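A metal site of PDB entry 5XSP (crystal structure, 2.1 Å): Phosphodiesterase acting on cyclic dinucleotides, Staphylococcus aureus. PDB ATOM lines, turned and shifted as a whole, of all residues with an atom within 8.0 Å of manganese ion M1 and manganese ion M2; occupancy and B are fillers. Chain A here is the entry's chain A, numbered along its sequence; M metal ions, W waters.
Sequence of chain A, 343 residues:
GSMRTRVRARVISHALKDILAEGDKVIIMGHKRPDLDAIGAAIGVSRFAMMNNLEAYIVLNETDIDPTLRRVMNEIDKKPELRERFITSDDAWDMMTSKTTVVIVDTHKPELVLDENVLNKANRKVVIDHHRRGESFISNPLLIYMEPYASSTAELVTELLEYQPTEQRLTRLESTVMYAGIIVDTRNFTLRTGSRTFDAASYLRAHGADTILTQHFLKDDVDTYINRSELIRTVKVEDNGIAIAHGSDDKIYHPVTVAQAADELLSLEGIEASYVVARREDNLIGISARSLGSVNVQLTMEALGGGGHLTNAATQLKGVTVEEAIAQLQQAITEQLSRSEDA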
ATOM      1  N   GLY A  30      -9.221   2.279  14.932  1.00  0.00           N
ATOM      2  CA  GLY A  30      -8.030   2.796  14.306  1.00  0.00           C
ATOM      3  C   GLY A  30      -7.624   1.928  13.116  1.00  0.00           C
ATOM      4  O   GLY A  30      -8.477   1.355  12.430  1.00  0.00           O
ATOM      5  N   HIS A  31      -6.326   1.830  12.873  1.00  0.00           N
ATOM      6  CA  HIS A  31      -5.800   1.059  11.757  1.00  0.00           C
ATOM      7  C   HIS A  31      -5.489  -0.404  12.116  1.00  0.00           C
ATOM      8  O   HIS A  31      -5.434  -0.768  13.285  1.00  0.00           O
ATOM      9  CB  HIS A  31      -4.543   1.745  11.188  1.00  0.00           C
ATOM     10  CG  HIS A  31      -3.481   2.009  12.207  1.00  0.00           C
ATOM     11  ND1 HIS A  31      -2.675   1.014  12.720  1.00  0.00           N
ATOM     12  CD2 HIS A  31      -3.076   3.160  12.800  1.00  0.00           C
ATOM     13  CE1 HIS A  31      -1.828   1.539  13.583  1.00  0.00           C
ATOM     14  NE2 HIS A  31      -2.052   2.841  13.656  1.00  0.00           N
ATOM     15  N   LYS A  32      -5.295  -1.244  11.101  1.00  0.00           N
ATOM     16  CA  LYS A  32      -4.967  -2.654  11.335  1.00  0.00           C
ATOM     17  C   LYS A  32      -3.643  -2.733  12.089  1.00  0.00           C
ATOM     18  O   LYS A  32      -2.780  -1.868  11.932  1.00  0.00           O
ATOM     19  CB  LYS A  32      -4.870  -3.409  10.008  1.00  0.00           C
ATOM     20  CG  LYS A  32      -6.197  -3.537   9.250  1.00  0.00           C
ATOM     21  CD  LYS A  32      -5.964  -3.885   7.775  1.00  0.00           C
ATOM     22  CE  LYS A  32      -7.112  -4.698   7.182  1.00  0.00           C
ATOM     23  NZ  LYS A  32      -8.450  -4.058   7.311  1.00  0.00           N
ATOM     24  N   ARG A  33      -3.489  -3.767  12.918  1.00  0.00           N
ATOM     25  CA  ARG A  33      -2.287  -3.906  13.733  1.00  0.00           C
ATOM     26  C   ARG A  33      -2.026  -2.596  14.504  1.00  0.00           C
ATOM     27  O   ARG A  33      -0.984  -1.966  14.339  1.00  0.00           O
ATOM     28  CB  ARG A  33      -1.098  -4.250  12.842  1.00  0.00           C
ATOM     29  CG  ARG A  33      -0.603  -5.686  13.015  1.00  0.00           C
ATOM     30  CD  ARG A  33       0.594  -5.730  13.958  1.00  0.00           C
ATOM     31  NE  ARG A  33       1.073  -7.085  14.219  1.00  0.00           N
ATOM     32  CZ  ARG A  33       2.190  -7.362  14.880  1.00  0.00           C
ATOM     33  NH1 ARG A  33       2.953  -6.361  15.329  1.00  0.00           N
ATOM     34  NH2 ARG A  33       2.564  -8.621  15.104  1.00  0.00           N
ATOM     35  N   PRO A  34      -2.994  -2.201  15.347  1.00  0.00           N
ATOM     36  CA  PRO A  34      -2.952  -0.864  15.950  1.00  0.00           C
ATOM     37  C   PRO A  34      -1.752  -0.687  16.873  1.00  0.00           C
ATOM     38  O   PRO A  34      -1.406  -1.594  17.640  1.00  0.00           O
ATOM     39  CB  PRO A  34      -4.248  -0.820  16.750  1.00  0.00           C
ATOM     40  CG  PRO A  34      -4.585  -2.275  17.035  1.00  0.00           C
ATOM     41  CD  PRO A  34      -4.125  -3.015  15.830  1.00  0.00           C
ATOM     42  N   ASP A  35      -1.084   0.467  16.780  1.00  0.00           N
ATOM     43  CA  ASP A  35      -0.028   0.803  17.718  1.00  0.00           C
ATOM     44  C   ASP A  35      -0.626   1.614  18.880  1.00  0.00           C
ATOM     45  O   ASP A  35      -1.850   1.764  18.975  1.00  0.00           O
ATOM     46  CB  ASP A  35       1.093   1.574  17.023  1.00  0.00           C
ATOM     47  CG  ASP A  35       0.582   2.793  16.278  1.00  0.00           C
ATOM     48  OD1 ASP A  35      -0.508   3.310  16.626  1.00  0.00           O
ATOM     49  OD2 ASP A  35       1.259   3.238  15.339  1.00  0.00           O
ATOM     50  N   LEU A  36       0.231   2.124  19.750  1.00  0.00           N
ATOM     51  CA  LEU A  36      -0.276   2.750  20.962  1.00  0.00           C
ATOM     52  C   LEU A  36      -0.897   4.126  20.720  1.00  0.00           C
ATOM     53  O   LEU A  36      -1.719   4.584  21.504  1.00  0.00           O
ATOM     54  CB  LEU A  36       0.805   2.797  22.061  1.00  0.00           C
ATOM     55  CG  LEU A  36       1.227   1.410  22.571  1.00  0.00           C
ATOM     56  CD1 LEU A  36       2.226   1.520  23.696  1.00  0.00           C
ATOM     57  CD2 LEU A  36       0.018   0.573  22.998  1.00  0.00           C
ATOM     58  N   ASP A  37      -0.526   4.811  19.644  1.00  0.00           N
ATOM     59  CA  ASP A  37      -1.215   6.055  19.316  1.00  0.00           C
ATOM     60  C   ASP A  37      -2.651   5.747  18.909  1.00  0.00           C
ATOM     61  O   ASP A  37      -3.576   6.411  19.352  1.00  0.00           O
ATOM     62  CB  ASP A  37      -0.495   6.842  18.216  1.00  0.00           C
ATOM     63  CG  ASP A  37      -1.092   8.237  18.033  1.00  0.00           C
ATOM     64  OD1 ASP A  37      -1.503   8.853  19.046  1.00  0.00           O
ATOM     65  OD2 ASP A  37      -1.130   8.735  16.883  1.00  0.00           O
ATOM     66  N   ALA A  38      -2.830   4.731  18.063  1.00  0.00           N
ATOM     67  CA  ALA A  38      -4.163   4.356  17.619  1.00  0.00           C
ATOM     68  C   ALA A  38      -5.009   3.976  18.836  1.00  0.00           C
ATOM     69  O   ALA A  38      -6.135   4.425  18.982  1.00  0.00           O
ATOM     70  CB  ALA A  38      -4.106   3.194  16.613  1.00  0.00           C
ATOM     71  N   ILE A  39      -4.441   3.164  19.726  1.00  0.00           N
ATOM     72  CA  ILE A  39      -5.194   2.704  20.867  1.00  0.00           C
ATOM     73  C   ILE A  39      -5.409   3.862  21.884  1.00  0.00           C
ATOM     74  O   ILE A  39      -6.490   4.050  22.411  1.00  0.00           O
ATOM     75  CB  ILE A  39      -4.519   1.494  21.499  1.00  0.00           C
ATOM     76  CG1 ILE A  39      -4.582   0.308  20.517  1.00  0.00           C
ATOM     77  CG2 ILE A  39      -5.173   1.141  22.817  1.00  0.00           C
ATOM     78  CD1 ILE A  39      -6.006  -0.187  20.207  1.00  0.00           C
ATOM     79  N   ALA A  41      -5.456   7.164  21.239  1.00  0.00           N
ATOM     80  CA  ALA A  41      -6.473   8.020  20.626  1.00  0.00           C
ATOM     81  C   ALA A  41      -7.876   7.454  20.837  1.00  0.00           C
ATOM     82  O   ALA A  41      -8.797   8.181  21.195  1.00  0.00           O
ATOM     83  CB  ALA A  41      -6.186   8.200  19.153  1.00  0.00           C
ATOM     84  N   VAL A 105      -9.759   6.794  14.010  1.00  0.00           N
ATOM     85  CA  VAL A 105      -8.604   7.526  14.557  1.00  0.00           C
ATOM     86  C   VAL A 105      -7.283   7.014  13.996  1.00  0.00           C
ATOM     87  O   VAL A 105      -7.089   5.794  13.815  1.00  0.00           O
ATOM     88  CB  VAL A 105      -8.539   7.392  16.095  1.00  0.00           C
ATOM     89  CG1 VAL A 105      -9.782   8.028  16.737  1.00  0.00           C
ATOM     90  CG2 VAL A 105      -8.450   5.921  16.486  1.00  0.00           C
ATOM     91  N   ASP A 106      -6.395   7.953  13.695  1.00  0.00           N
ATOM     92  CA  ASP A 106      -5.004   7.661  13.375  1.00  0.00           C
ATOM     93  C   ASP A 106      -4.830   6.957  12.031  1.00  0.00           C
ATOM     94  O   ASP A 106      -3.778   6.361  11.750  1.00  0.00           O
ATOM     95  CB  ASP A 106      -4.361   6.853  14.498  1.00  0.00           C
ATOM     96  CG  ASP A 106      -2.871   7.006  14.508  1.00  0.00           C
ATOM     97  OD1 ASP A 106      -2.389   8.131  14.273  1.00  0.00           O
ATOM     98  OD2 ASP A 106      -2.198   6.001  14.744  1.00  0.00           O
ATOM     99  N   THR A 107      -5.858   7.048  11.207  1.00  0.00           N
ATOM    100  CA  THR A 107      -5.744   6.696   9.802  1.00  0.00           C
ATOM    101  C   THR A 107      -6.896   7.372   9.067  1.00  0.00           C
ATOM    102  O   THR A 107      -7.845   7.834   9.704  1.00  0.00           O
ATOM    103  CB  THR A 107      -5.809   5.173   9.614  1.00  0.00           C
ATOM    104  OG1 THR A 107      -5.533   4.862   8.243  1.00  0.00           O
ATOM    105  CG2 THR A 107      -7.163   4.666   9.990  1.00  0.00           C
ATOM    106  N   ASP A 129      -7.030  12.445  12.448  1.00  0.00           N
ATOM    107  CA  ASP A 129      -5.731  11.902  12.065  1.00  0.00           C
ATOM    108  C   ASP A 129      -4.715  13.023  11.927  1.00  0.00           C
ATOM    109  O   ASP A 129      -5.098  14.184  11.802  1.00  0.00           O
ATOM    110  CB  ASP A 129      -5.872  11.112  10.762  1.00  0.00           C
ATOM    111  CG  ASP A 129      -4.610  10.367  10.377  1.00  0.00           C
ATOM    112  OD1 ASP A 129      -3.813   9.970  11.256  1.00  0.00           O
ATOM    113  OD2 ASP A 129      -4.433  10.172   9.168  1.00  0.00           O
ATOM    114  N   HIS A 130      -3.431  12.685  11.946  1.00  0.00           N
ATOM    115  CA  HIS A 130      -2.362  13.684  11.911  1.00  0.00           C
ATOM    116  C   HIS A 130      -1.441  13.495  10.703  1.00  0.00           C
ATOM    117  O   HIS A 130      -0.269  13.855  10.736  1.00  0.00           O
ATOM    118  CB  HIS A 130      -1.555  13.683  13.213  1.00  0.00           C
ATOM    119  CG  HIS A 130      -0.776  12.424  13.444  1.00  0.00           C
ATOM    120  ND1 HIS A 130       0.597  12.381  13.405  1.00  0.00           N
ATOM    121  CD2 HIS A 130      -1.188  11.160  13.748  1.00  0.00           C
ATOM    122  CE1 HIS A 130       1.006  11.145  13.659  1.00  0.00           C
ATOM    123  NE2 HIS A 130      -0.052  10.396  13.862  1.00  0.00           N
ATOM    124  N   HIS A 131      -1.965  12.910   9.642  1.00  0.00           N
ATOM    125  CA  HIS A 131      -1.218  12.862   8.398  1.00  0.00           C
ATOM    126  C   HIS A 131      -1.984  13.697   7.386  1.00  0.00           C
ATOM    127  O   HIS A 131      -3.122  14.099   7.635  1.00  0.00           O
ATOM    128  CB  HIS A 131      -1.063  11.409   7.936  1.00  0.00           C
ATOM    129  CG  HIS A 131      -0.848  10.440   9.064  1.00  0.00           C
ATOM    130  ND1 HIS A 131       0.256  10.466   9.874  1.00  0.00           N
ATOM    131  CD2 HIS A 131      -1.617   9.411   9.504  1.00  0.00           C
ATOM    132  CE1 HIS A 131       0.174   9.499  10.778  1.00  0.00           C
ATOM    133  NE2 HIS A 131      -0.962   8.852  10.573  1.00  0.00           N
ATOM    134  N   ALA A 150       0.605  17.930  13.851  1.00  0.00           N
ATOM    135  CA  ALA A 150       0.478  17.402  15.209  1.00  0.00           C
ATOM    136  C   ALA A 150       1.343  16.159  15.386  1.00  0.00           C
ATOM    137  O   ALA A 150       1.563  15.415  14.435  1.00  0.00           O
ATOM    138  CB  ALA A 150      -0.981  17.075  15.516  1.00  0.00           C
ATOM    139  N   SER A 151       1.835  15.905  16.595  1.00  0.00           N
ATOM    140  CA  SER A 151       2.719  14.759  16.819  1.00  0.00           C
ATOM    141  C   SER A 151       2.035  13.426  16.581  1.00  0.00           C
ATOM    142  O   SER A 151       2.656  12.452  16.174  1.00  0.00           O
ATOM    143  CB  SER A 151       3.289  14.760  18.248  1.00  0.00           C
ATOM    144  OG  SER A 151       2.259  14.628  19.213  1.00  0.00           O
ATOM    145  N   SER A 152       0.728  13.375  16.845  1.00  0.00           N
ATOM    146  CA  SER A 152       0.043  12.109  17.020  1.00  0.00           C
ATOM    147  C   SER A 152      -1.436  12.349  17.104  1.00  0.00           C
ATOM    148  O   SER A 152      -1.876  13.486  17.299  1.00  0.00           O
ATOM    149  CB  SER A 152       0.497  11.462  18.328  1.00  0.00           C
ATOM    150  OG  SER A 152       0.327  12.399  19.383  1.00  0.00           O
ATOM    151  N   THR A 153      -2.217  11.282  16.968  1.00  0.00           N
ATOM    152  CA  THR A 153      -3.654  11.423  17.135  1.00  0.00           C
ATOM    153  C   THR A 153      -3.963  11.619  18.627  1.00  0.00           C
ATOM    154  O   THR A 153      -4.912  12.315  18.982  1.00  0.00           O
ATOM    155  CB  THR A 153      -4.407  10.233  16.513  1.00  0.00           C
ATOM    156  OG1 THR A 153      -3.974  10.097  15.148  1.00  0.00           O
ATOM    157  CG2 THR A 153      -5.937  10.431  16.548  1.00  0.00           C
ATOM    158  N   ALA A 154      -3.138  11.032  19.496  1.00  0.00           N
ATOM    159  CA  ALA A 154      -3.364  11.179  20.936  1.00  0.00           C
ATOM    160  C   ALA A 154      -3.316  12.649  21.330  1.00  0.00           C
ATOM    161  O   ALA A 154      -4.128  13.126  22.118  1.00  0.00           O
ATOM    162  CB  ALA A 154      -2.345  10.367  21.746  1.00  0.00           C
ATOM    163  N   GLY A 181       1.239   6.620  23.581  1.00  0.00           N
ATOM    164  CA  GLY A 181       1.068   6.850  22.145  1.00  0.00           C
ATOM    165  C   GLY A 181       1.835   8.065  21.673  1.00  0.00           C
ATOM    166  O   GLY A 181       2.425   8.064  20.576  1.00  0.00           O
ATOM    167  N   ILE A 182       1.823   9.125  22.459  1.00  0.00           N
ATOM    168  CA  ILE A 182       2.604  10.303  22.105  1.00  0.00           C
ATOM    169  C   ILE A 182       4.103   9.982  22.146  1.00  0.00           C
ATOM    170  O   ILE A 182       4.834  10.347  21.236  1.00  0.00           O
ATOM    171  CB  ILE A 182       2.288  11.504  22.999  1.00  0.00           C
ATOM    172  CG1 ILE A 182       0.815  11.892  22.850  1.00  0.00           C
ATOM    173  CG2 ILE A 182       3.210  12.674  22.659  1.00  0.00           C
ATOM    174  CD1 ILE A 182       0.425  13.146  23.577  1.00  0.00           C
ATOM    175  N   VAL A 184       5.559   7.187  21.617  1.00  0.00           N
ATOM    176  CA  VAL A 184       5.951   6.358  20.474  1.00  0.00           C
ATOM    177  C   VAL A 184       6.037   7.186  19.189  1.00  0.00           C
ATOM    178  O   VAL A 184       7.052   7.165  18.512  1.00  0.00           O
ATOM    179  CB  VAL A 184       4.993   5.168  20.255  1.00  0.00           C
ATOM    180  CG1 VAL A 184       5.361   4.406  18.962  1.00  0.00           C
ATOM    181  CG2 VAL A 184       5.045   4.224  21.435  1.00  0.00           C
ATOM    182  N   ASP A 185       4.990   7.928  18.885  1.00  0.00           N
ATOM    183  CA  ASP A 185       4.970   8.723  17.669  1.00  0.00           C
ATOM    184  C   ASP A 185       6.047   9.813  17.629  1.00  0.00           C
ATOM    185  O   ASP A 185       6.461  10.234  16.582  1.00  0.00           O
ATOM    186  CB  ASP A 185       3.599   9.330  17.477  1.00  0.00           C
ATOM    187  CG  ASP A 185       2.674   8.409  16.712  1.00  0.00           C
ATOM    188  OD1 ASP A 185       2.992   7.227  16.555  1.00  0.00           O
ATOM    189  OD2 ASP A 185       1.622   8.886  16.281  1.00  0.00           O
ATOM    190  N   THR A 186       6.496  10.282  18.786  1.00  0.00           N
ATOM    191  CA  THR A 186       7.498  11.342  18.833  1.00  0.00           C
ATOM    192  C   THR A 186       8.921  10.842  19.104  1.00  0.00           C
ATOM    193  O   THR A 186       9.846  11.627  19.098  1.00  0.00           O
ATOM    194  CB  THR A 186       7.162  12.426  19.879  1.00  0.00           C
ATOM    195  OG1 THR A 186       7.193  11.845  21.185  1.00  0.00           O
ATOM    196  CG2 THR A 186       5.812  13.030  19.653  1.00  0.00           C
ATOM    197  N   ARG A 192       8.604  15.760  15.630  1.00  0.00           N
ATOM    198  CA  ARG A 192       7.250  16.300  15.490  1.00  0.00           C
ATOM    199  C   ARG A 192       6.672  16.802  16.801  1.00  0.00           C
ATOM    200  O   ARG A 192       5.484  16.647  17.089  1.00  0.00           O
ATOM    201  CB  ARG A 192       6.320  15.246  14.877  1.00  0.00           C
ATOM    202  CG  ARG A 192       6.690  14.862  13.442  1.00  0.00           C
ATOM    203  CD  ARG A 192       5.748  13.781  12.870  1.00  0.00           C
ATOM    204  NE  ARG A 192       4.412  14.310  12.602  1.00  0.00           N
ATOM    205  CZ  ARG A 192       3.402  13.584  12.118  1.00  0.00           C
ATOM    206  NH1 ARG A 192       3.578  12.295  11.840  1.00  0.00           N
ATOM    207  NH2 ARG A 192       2.214  14.141  11.901  1.00  0.00           N
HETATM  208 MN    MN M   1      -0.329   4.708  14.064  1.00  0.00          MN
HETATM  209 MN    MN M   2      -0.098   8.114  14.967  1.00  0.00          MN
HETATM  210  O   HOH W   1       1.287   6.102  15.088  1.00  0.00           O
HETATM  211  O   HOH W   2       2.039   7.498  12.846  1.00  0.00           O
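The backbone NH of Asp 37 lies close to the side-chain carboxylate of Asp 35 (3.4 Å). N of Thr 153 is in hydrogen-bond range of OD1 of Asp 37 (3.3 Å). The backbone NH of Ala 154 sits at hydrogen-bond distance from the side-chain carboxylate of Asp 37 (2.8 Å). The side-chain carboxylate of Asp 106 sits close to the side-chain hydroxyl of Thr 153 (2.7 Å). OD1 of Asp 35 is in hydrogen-bond range of N of Ala 38 (3.1 Å). O of Ser 151 lies close to ND1 of His 130, at 3.5 Å. The backbone carbonyl oxygen (O) of His 130 lies within hydrogen-bond range of the guanidinium group (NH2) of Arg 192 (2.8 Å). A ring nitrogen (ND1) of His 130 sits at hydrogen-bond distance from the backbone carbonyl oxygen (O) of Ala 150 (3.3 Å).
Within 4 Å of manganese ion M1: His 31, Asp 35 and Asp 106. The nearest printed residue that does not touch manganese ion M1 is Asp 37 (4.7 Å).
The nearest printed residue that does not touch manganese ion M2 is Thr 153 (4.3 Å).
Water W1 binds manganese ion M1, at 2.4 Å. Manganese ion M1 is bound by OD2 of Asp 106 (2.4 Å). Manganese ion M1 is bound by OD2 of Asp 35 (2.5 Å). Manganese ion M1 is bound by NE2 of His 31, at 2.6 Å. Slightly farther from manganese ion M1 lies the side-chain carboxylate (OD1) of Asp 35 (2.9 Å).
Manganese ion M2 is bound by OD2 of Asp 37 (2.3 Å), OD2 of Asp 185 (2.3 Å), OD1 of Asp 106 (2.4 Å), water W1 (2.4 Å) and NE2 of His 130 (2.5 Å).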
